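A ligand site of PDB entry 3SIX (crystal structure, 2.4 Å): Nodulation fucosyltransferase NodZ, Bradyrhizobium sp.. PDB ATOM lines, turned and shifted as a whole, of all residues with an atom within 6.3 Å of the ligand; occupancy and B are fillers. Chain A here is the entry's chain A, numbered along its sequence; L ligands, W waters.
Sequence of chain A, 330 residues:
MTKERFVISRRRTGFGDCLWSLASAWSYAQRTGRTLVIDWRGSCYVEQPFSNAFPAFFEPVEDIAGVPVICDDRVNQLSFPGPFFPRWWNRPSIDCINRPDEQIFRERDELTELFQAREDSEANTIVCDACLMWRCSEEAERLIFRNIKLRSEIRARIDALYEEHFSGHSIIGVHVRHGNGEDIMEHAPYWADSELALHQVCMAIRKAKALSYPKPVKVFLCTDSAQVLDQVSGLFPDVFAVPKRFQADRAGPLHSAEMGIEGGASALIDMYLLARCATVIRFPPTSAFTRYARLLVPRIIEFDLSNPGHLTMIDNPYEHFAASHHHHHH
N4 of the ligand lies close to N of Ala 267, at 3.5 Å.
CA of Gly 14 touches O10 of the ligand, at 3.5 Å.
Cys 222 touches the ligand.
Ser 266 touches the ligand (OG to N4, 3.7 Å).
CZ of Phe 289 touches C8 of the ligand, 3.5 Å away.
Hydrophobic or aromatic side chains within 4 Å of the ligand: His 175, Ala 267 and Phe 289.
Nine residues have an atom within 4 Å of the ligand: Gly 14, Tyr 45, His 175, Arg 177, Cys 222, Ser 266, Ala 267, Asp 270 and Phe 289.
The nearest printed residue that does not touch the ligand is Phe 15 (4.3 Å).
Water W1 bridges the backbone NH (N) of Gly 16 (3.0 Å) and an oxygen (O10) of the ligand (3.3 Å).
The side-chain sulfur (SG) of Cys 222 sits close to the side-chain carboxylate (OD2) of Asp 270 (3.7 Å).
O of Cys 222 lies within hydrogen-bond range of N of Val 176, at 3.0 Å.
N of Phe 289 lies close to OG of Ser 287, 3.5 Å away.
The side-chain carboxylate (OD1) of Asp 224 is in salt-bridge range of the guanidinium group (NH2) of Arg 177, 3.0 Å away.
The side-chain hydroxyl (OH) of Tyr 45 lies within hydrogen-bond range of an oxygen (O9) of the ligand (3.3 Å).
The guanidinium group (NH1) of Arg 177 sits at hydrogen-bond distance from a nitrogen (N2) of the ligand, at 3.1 Å.
A nitrogen (N3) of the ligand is in hydrogen-bond range of the side-chain carboxylate (OD2) of Asp 270, 3.0 Å away.
A nitrogen (N2) of the ligand is in hydrogen-bond range of a ring nitrogen (NE2) of His 175 (2.8 Å).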
ATOM      1  N   THR A  13       6.486  14.456  17.522  1.00  0.00           N
ATOM      2  CA  THR A  13       6.927  14.159  16.135  1.00  0.00           C
ATOM      3  C   THR A  13       8.462  14.121  16.147  1.00  0.00           C
ATOM      4  O   THR A  13       9.057  13.917  17.202  1.00  0.00           O
ATOM      5  CB  THR A  13       6.425  15.238  15.138  1.00  0.00           C
ATOM      6  OG1 THR A  13       6.835  16.526  15.616  1.00  0.00           O
ATOM      7  CG2 THR A  13       4.902  15.216  14.980  1.00  0.00           C
ATOM      8  N   GLY A  14       9.105  14.389  15.005  1.00  0.00           N
ATOM      9  CA  GLY A  14      10.583  14.415  14.950  1.00  0.00           C
ATOM     10  C   GLY A  14      11.161  15.464  15.893  1.00  0.00           C
ATOM     11  O   GLY A  14      10.484  16.461  16.232  1.00  0.00           O
ATOM     12  N   PHE A  15      12.387  15.233  16.330  1.00  0.00           N
ATOM     13  CA  PHE A  15      13.049  16.081  17.317  1.00  0.00           C
ATOM     14  C   PHE A  15      13.265  17.523  16.853  1.00  0.00           C
ATOM     15  O   PHE A  15      13.268  18.408  17.679  1.00  0.00           O
ATOM     16  CB  PHE A  15      14.387  15.461  17.732  1.00  0.00           C
ATOM     17  CG  PHE A  15      14.235  14.243  18.606  1.00  0.00           C
ATOM     18  CD1 PHE A  15      13.670  14.331  19.859  1.00  0.00           C
ATOM     19  CD2 PHE A  15      14.693  13.047  18.186  1.00  0.00           C
ATOM     20  CE1 PHE A  15      13.519  13.199  20.652  1.00  0.00           C
ATOM     21  CE2 PHE A  15      14.566  11.925  18.963  1.00  0.00           C
ATOM     22  CZ  PHE A  15      13.975  11.992  20.204  1.00  0.00           C
ATOM     23  N   GLY A  16      13.475  17.755  15.559  1.00  0.00           N
ATOM     24  CA  GLY A  16      13.666  19.130  15.094  1.00  0.00           C
ATOM     25  C   GLY A  16      12.412  19.986  15.366  1.00  0.00           C
ATOM     26  O   GLY A  16      12.517  21.148  15.826  1.00  0.00           O
ATOM     27  N   CYS A  44       6.657   9.574  19.093  1.00  0.00           N
ATOM     28  CA  CYS A  44       6.756   8.510  18.091  1.00  0.00           C
ATOM     29  C   CYS A  44       7.915   7.552  18.405  1.00  0.00           C
ATOM     30  O   CYS A  44       7.962   6.436  17.876  1.00  0.00           O
ATOM     31  CB  CYS A  44       6.921   9.094  16.689  1.00  0.00           C
ATOM     32  SG  CYS A  44       8.354  10.183  16.502  1.00  0.00           S
ATOM     33  N   TYR A  45       8.829   7.997  19.253  1.00  0.00           N
ATOM     34  CA  TYR A  45      10.008   7.193  19.649  1.00  0.00           C
ATOM     35  C   TYR A  45       9.854   6.347  20.898  1.00  0.00           C
ATOM     36  O   TYR A  45      10.772   5.630  21.239  1.00  0.00           O
ATOM     37  CB  TYR A  45      11.198   8.114  19.868  1.00  0.00           C
ATOM     38  CG  TYR A  45      11.575   8.867  18.649  1.00  0.00           C
ATOM     39  CD1 TYR A  45      12.016   8.184  17.528  1.00  0.00           C
ATOM     40  CD2 TYR A  45      11.430  10.229  18.580  1.00  0.00           C
ATOM     41  CE1 TYR A  45      12.328   8.830  16.395  1.00  0.00           C
ATOM     42  CE2 TYR A  45      11.768  10.905  17.409  1.00  0.00           C
ATOM     43  CZ  TYR A  45      12.198  10.183  16.325  1.00  0.00           C
ATOM     44  OH  TYR A  45      12.535  10.776  15.143  1.00  0.00           O
ATOM     45  N   HIS A 175      21.834  15.699   4.031  1.00  0.00           N
ATOM     46  CA  HIS A 175      20.595  15.193   4.554  1.00  0.00           C
ATOM     47  C   HIS A 175      19.660  14.961   3.404  1.00  0.00           C
ATOM     48  O   HIS A 175      19.282  15.937   2.736  1.00  0.00           O
ATOM     49  CB  HIS A 175      19.931  16.181   5.523  1.00  0.00           C
ATOM     50  CG  HIS A 175      18.658  15.663   6.121  1.00  0.00           C
ATOM     51  ND1 HIS A 175      17.439  16.271   5.909  1.00  0.00           N
ATOM     52  CD2 HIS A 175      18.410  14.544   6.852  1.00  0.00           C
ATOM     53  CE1 HIS A 175      16.506  15.581   6.553  1.00  0.00           C
ATOM     54  NE2 HIS A 175      17.062  14.526   7.121  1.00  0.00           N
ATOM     55  N   VAL A 176      19.270  13.714   3.185  1.00  0.00           N
ATOM     56  CA  VAL A 176      18.437  13.345   2.031  1.00  0.00           C
ATOM     57  C   VAL A 176      17.170  12.654   2.520  1.00  0.00           C
ATOM     58  O   VAL A 176      17.229  11.524   2.989  1.00  0.00           O
ATOM     59  CB  VAL A 176      19.191  12.350   1.080  1.00  0.00           C
ATOM     60  CG1 VAL A 176      18.257  11.897  -0.084  1.00  0.00           C
ATOM     61  CG2 VAL A 176      20.488  12.956   0.568  1.00  0.00           C
ATOM     62  N   ARG A 177      16.046  13.326   2.449  1.00  0.00           N
ATOM     63  CA  ARG A 177      14.796  12.718   2.897  1.00  0.00           C
ATOM     64  C   ARG A 177      14.114  12.096   1.691  1.00  0.00           C
ATOM     65  O   ARG A 177      13.859  12.778   0.680  1.00  0.00           O
ATOM     66  CB  ARG A 177      13.905  13.732   3.622  1.00  0.00           C
ATOM     67  CG  ARG A 177      13.171  13.169   4.854  1.00  0.00           C
ATOM     68  CD  ARG A 177      14.067  12.362   5.802  1.00  0.00           C
ATOM     69  NE  ARG A 177      13.418  11.137   6.296  1.00  0.00           N
ATOM     70  CZ  ARG A 177      14.040  10.114   6.886  1.00  0.00           C
ATOM     71  NH1 ARG A 177      15.370  10.098   7.056  1.00  0.00           N
ATOM     72  NH2 ARG A 177      13.321   9.072   7.307  1.00  0.00           N
ATOM     73  N   HIS A 178      13.858  10.791   1.821  1.00  0.00           N
ATOM     74  CA  HIS A 178      13.493   9.863   0.719  1.00  0.00           C
ATOM     75  C   HIS A 178      14.727   9.519  -0.146  1.00  0.00           C
ATOM     76  O   HIS A 178      14.730   9.588  -1.389  1.00  0.00           O
ATOM     77  CB  HIS A 178      12.287  10.381  -0.083  1.00  0.00           C
ATOM     78  CG  HIS A 178      11.074  10.637   0.764  1.00  0.00           C
ATOM     79  ND1 HIS A 178       9.796  10.610   0.253  1.00  0.00           N
ATOM     80  CD2 HIS A 178      10.939  10.897   2.093  1.00  0.00           C
ATOM     81  CE1 HIS A 178       8.923  10.850   1.217  1.00  0.00           C
ATOM     82  NE2 HIS A 178       9.592  11.038   2.343  1.00  0.00           N
ATOM     83  N   CYS A 222      23.324  11.327   5.477  1.00  0.00           N
ATOM     84  CA  CYS A 222      22.215  10.966   6.385  1.00  0.00           C
ATOM     85  C   CYS A 222      20.963  10.733   5.554  1.00  0.00           C
ATOM     86  O   CYS A 222      20.322  11.668   5.071  1.00  0.00           O
ATOM     87  CB  CYS A 222      21.948  12.074   7.389  1.00  0.00           C
ATOM     88  SG  CYS A 222      23.257  12.369   8.601  1.00  0.00           S
ATOM     89  N   THR A 223      20.648   9.476   5.325  1.00  0.00           N
ATOM     90  CA  THR A 223      19.541   9.075   4.499  1.00  0.00           C
ATOM     91  C   THR A 223      18.927   7.784   5.063  1.00  0.00           C
ATOM     92  O   THR A 223      19.607   6.972   5.709  1.00  0.00           O
ATOM     93  CB  THR A 223      20.032   8.839   3.052  1.00  0.00           C
ATOM     94  OG1 THR A 223      18.928   8.472   2.193  1.00  0.00           O
ATOM     95  CG2 THR A 223      21.073   7.742   3.022  1.00  0.00           C
ATOM     96  N   ASP A 224      17.646   7.576   4.762  1.00  0.00           N
ATOM     97  CA  ASP A 224      16.922   6.374   5.177  1.00  0.00           C
ATOM     98  C   ASP A 224      17.004   5.239   4.129  1.00  0.00           C
ATOM     99  O   ASP A 224      16.675   4.053   4.405  1.00  0.00           O
ATOM    100  CB  ASP A 224      15.444   6.698   5.468  1.00  0.00           C
ATOM    101  CG  ASP A 224      14.772   7.598   4.381  1.00  0.00           C
ATOM    102  OD1 ASP A 224      13.559   7.882   4.554  1.00  0.00           O
ATOM    103  OD2 ASP A 224      15.424   8.021   3.397  1.00  0.00           O
ATOM    104  N   GLY A 263      15.725   4.245  17.478  1.00  0.00           N
ATOM    105  CA  GLY A 263      15.367   5.213  16.423  1.00  0.00           C
ATOM    106  C   GLY A 263      15.534   6.688  16.875  1.00  0.00           C
ATOM    107  O   GLY A 263      16.064   7.515  16.148  1.00  0.00           O
ATOM    108  N   SER A 266      19.409   7.398  17.240  1.00  0.00           N
ATOM    109  CA  SER A 266      20.135   7.586  15.969  1.00  0.00           C
ATOM    110  C   SER A 266      19.683   8.858  15.212  1.00  0.00           C
ATOM    111  O   SER A 266      20.526   9.531  14.556  1.00  0.00           O
ATOM    112  CB  SER A 266      20.118   6.318  15.091  1.00  0.00           C
ATOM    113  OG  SER A 266      18.913   6.165  14.430  1.00  0.00           O
ATOM    114  N   ALA A 267      18.406   9.246  15.348  1.00  0.00           N
ATOM    115  CA  ALA A 267      17.946  10.537  14.814  1.00  0.00           C
ATOM    116  C   ALA A 267      18.738  11.711  15.452  1.00  0.00           C
ATOM    117  O   ALA A 267      19.244  12.581  14.770  1.00  0.00           O
ATOM    118  CB  ALA A 267      16.389  10.714  15.018  1.00  0.00           C
ATOM    119  N   LEU A 268      18.910  11.669  16.761  1.00  0.00           N
ATOM    120  CA  LEU A 268      19.668  12.734  17.473  1.00  0.00           C
ATOM    121  C   LEU A 268      21.138  12.699  17.130  1.00  0.00           C
ATOM    122  O   LEU A 268      21.793  13.745  17.064  1.00  0.00           O
ATOM    123  CB  LEU A 268      19.473  12.622  18.987  1.00  0.00           C
ATOM    124  CG  LEU A 268      18.067  12.960  19.487  1.00  0.00           C
ATOM    125  CD1 LEU A 268      17.847  12.432  20.950  1.00  0.00           C
ATOM    126  CD2 LEU A 268      17.711  14.468  19.395  1.00  0.00           C
ATOM    127  N   ASP A 270      22.567  11.771  14.241  1.00  0.00           N
ATOM    128  CA  ASP A 270      22.679  12.456  12.950  1.00  0.00           C
ATOM    129  C   ASP A 270      22.405  13.971  13.057  1.00  0.00           C
ATOM    130  O   ASP A 270      23.127  14.770  12.483  1.00  0.00           O
ATOM    131  CB  ASP A 270      21.694  11.869  11.972  1.00  0.00           C
ATOM    132  CG  ASP A 270      22.139  10.540  11.364  1.00  0.00           C
ATOM    133  OD1 ASP A 270      23.304  10.088  11.547  1.00  0.00           O
ATOM    134  OD2 ASP A 270      21.291   9.984  10.679  1.00  0.00           O
ATOM    135  N   MET A 271      21.357  14.353  13.771  1.00  0.00           N
ATOM    136  CA  MET A 271      20.983  15.775  13.864  1.00  0.00           C
ATOM    137  C   MET A 271      22.148  16.600  14.402  1.00  0.00           C
ATOM    138  O   MET A 271      22.490  17.701  13.854  1.00  0.00           O
ATOM    139  CB  MET A 271      19.787  15.933  14.773  1.00  0.00           C
ATOM    140  CG  MET A 271      18.977  17.168  14.606  1.00  0.00           C
ATOM    141  SD  MET A 271      17.307  16.990  15.373  1.00  0.00           S
ATOM    142  CE  MET A 271      17.723  17.885  16.793  1.00  0.00           C
ATOM    143  N   LEU A 274      25.332  16.582  12.014  1.00  0.00           N
ATOM    144  CA  LEU A 274      25.136  17.518  10.900  1.00  0.00           C
ATOM    145  C   LEU A 274      25.535  18.949  11.312  1.00  0.00           C
ATOM    146  O   LEU A 274      26.144  19.691  10.522  1.00  0.00           O
ATOM    147  CB  LEU A 274      23.715  17.457  10.347  1.00  0.00           C
ATOM    148  CG  LEU A 274      23.385  16.195   9.498  1.00  0.00           C
ATOM    149  CD1 LEU A 274      21.904  16.171   9.082  1.00  0.00           C
ATOM    150  CD2 LEU A 274      24.238  16.136   8.235  1.00  0.00           C
ATOM    151  N   SER A 287      12.885  20.714   5.957  1.00  0.00           N
ATOM    152  CA  SER A 287      12.995  19.813   7.097  1.00  0.00           C
ATOM    153  C   SER A 287      13.489  20.516   8.372  1.00  0.00           C
ATOM    154  O   SER A 287      14.547  21.121   8.366  1.00  0.00           O
ATOM    155  CB  SER A 287      14.011  18.692   6.793  1.00  0.00           C
ATOM    156  OG  SER A 287      13.761  17.579   7.619  1.00  0.00           O
ATOM    157  N   PHE A 289      14.616  18.859  10.721  1.00  0.00           N
ATOM    158  CA  PHE A 289      15.734  17.992  11.121  1.00  0.00           C
ATOM    159  C   PHE A 289      17.115  18.647  11.003  1.00  0.00           C
ATOM    160  O   PHE A 289      18.049  18.391  11.797  1.00  0.00           O
ATOM    161  CB  PHE A 289      15.716  16.686  10.312  1.00  0.00           C
ATOM    162  CG  PHE A 289      16.713  15.638  10.805  1.00  0.00           C
ATOM    163  CD1 PHE A 289      17.941  15.507  10.220  1.00  0.00           C
ATOM    164  CD2 PHE A 289      16.383  14.756  11.869  1.00  0.00           C
ATOM    165  CE1 PHE A 289      18.889  14.539  10.685  1.00  0.00           C
ATOM    166  CE2 PHE A 289      17.287  13.805  12.335  1.00  0.00           C
ATOM    167  CZ  PHE A 289      18.558  13.706  11.738  1.00  0.00           C
HETATM  168  P1  LIG L   1       7.577  14.281   9.439  1.00  0.00           P
HETATM  169  O1  LIG L   1       6.507  15.421   8.912  1.00  0.00           O
HETATM  170  O2  LIG L   1       7.135  13.750  10.763  1.00  0.00           O
HETATM  171  O3  LIG L   1       9.014  15.054   9.509  1.00  0.00           O
HETATM  172  O4  LIG L   1       7.683  13.101   8.214  1.00  0.00           O
HETATM  173  P2  LIG L   1       9.076  12.643   7.386  1.00  0.00           P
HETATM  174  O5  LIG L   1       9.070  11.136   7.282  1.00  0.00           O
HETATM  175  O6  LIG L   1       9.269  13.472   6.165  1.00  0.00           O
HETATM  176  O7  LIG L   1      10.280  13.048   8.451  1.00  0.00           O
HETATM  177  C1  LIG L   1      11.322  12.077   8.735  1.00  0.00           C
HETATM  178  C2  LIG L   1      11.195  11.320  10.094  1.00  0.00           C
HETATM  179  O8  LIG L   1      12.514  10.616  10.304  1.00  0.00           O
HETATM  180  C3  LIG L   1      11.100  12.334  11.223  1.00  0.00           C
HETATM  181  O9  LIG L   1      10.897  11.651  12.455  1.00  0.00           O
HETATM  182  C4  LIG L   1      12.528  12.836  11.179  1.00  0.00           C
HETATM  183  O10 LIG L   1      12.827  13.576  12.357  1.00  0.00           O
HETATM  184  C5  LIG L   1      13.351  11.516  11.074  1.00  0.00           C
HETATM  185  N1  LIG L   1      14.593  11.730  10.278  1.00  0.00           N
HETATM  186  C6  LIG L   1      14.715  12.640   9.297  1.00  0.00           C
HETATM  187  N2  LIG L   1      15.934  12.589   8.782  1.00  0.00           N
HETATM  188  C7  LIG L   1      16.615  11.653   9.470  1.00  0.00           C
HETATM  189  C8  LIG L   1      17.920  11.190   9.367  1.00  0.00           C
HETATM  190  O11 LIG L   1      18.674  11.690   8.521  1.00  0.00           O
HETATM  191  N3  LIG L   1      18.359  10.160  10.246  1.00  0.00           N
HETATM  192  C9  LIG L   1      17.454   9.630  11.151  1.00  0.00           C
HETATM  193  N4  LIG L   1      17.872   8.668  11.962  1.00  0.00           N
HETATM  194  N5  LIG L   1      16.203  10.124  11.220  1.00  0.00           N
HETATM  195  C10 LIG L   1      15.764  11.096  10.403  1.00  0.00           C
HETATM  196  O   HOH W   1      12.451  16.762  12.913  1.00  0.00           O
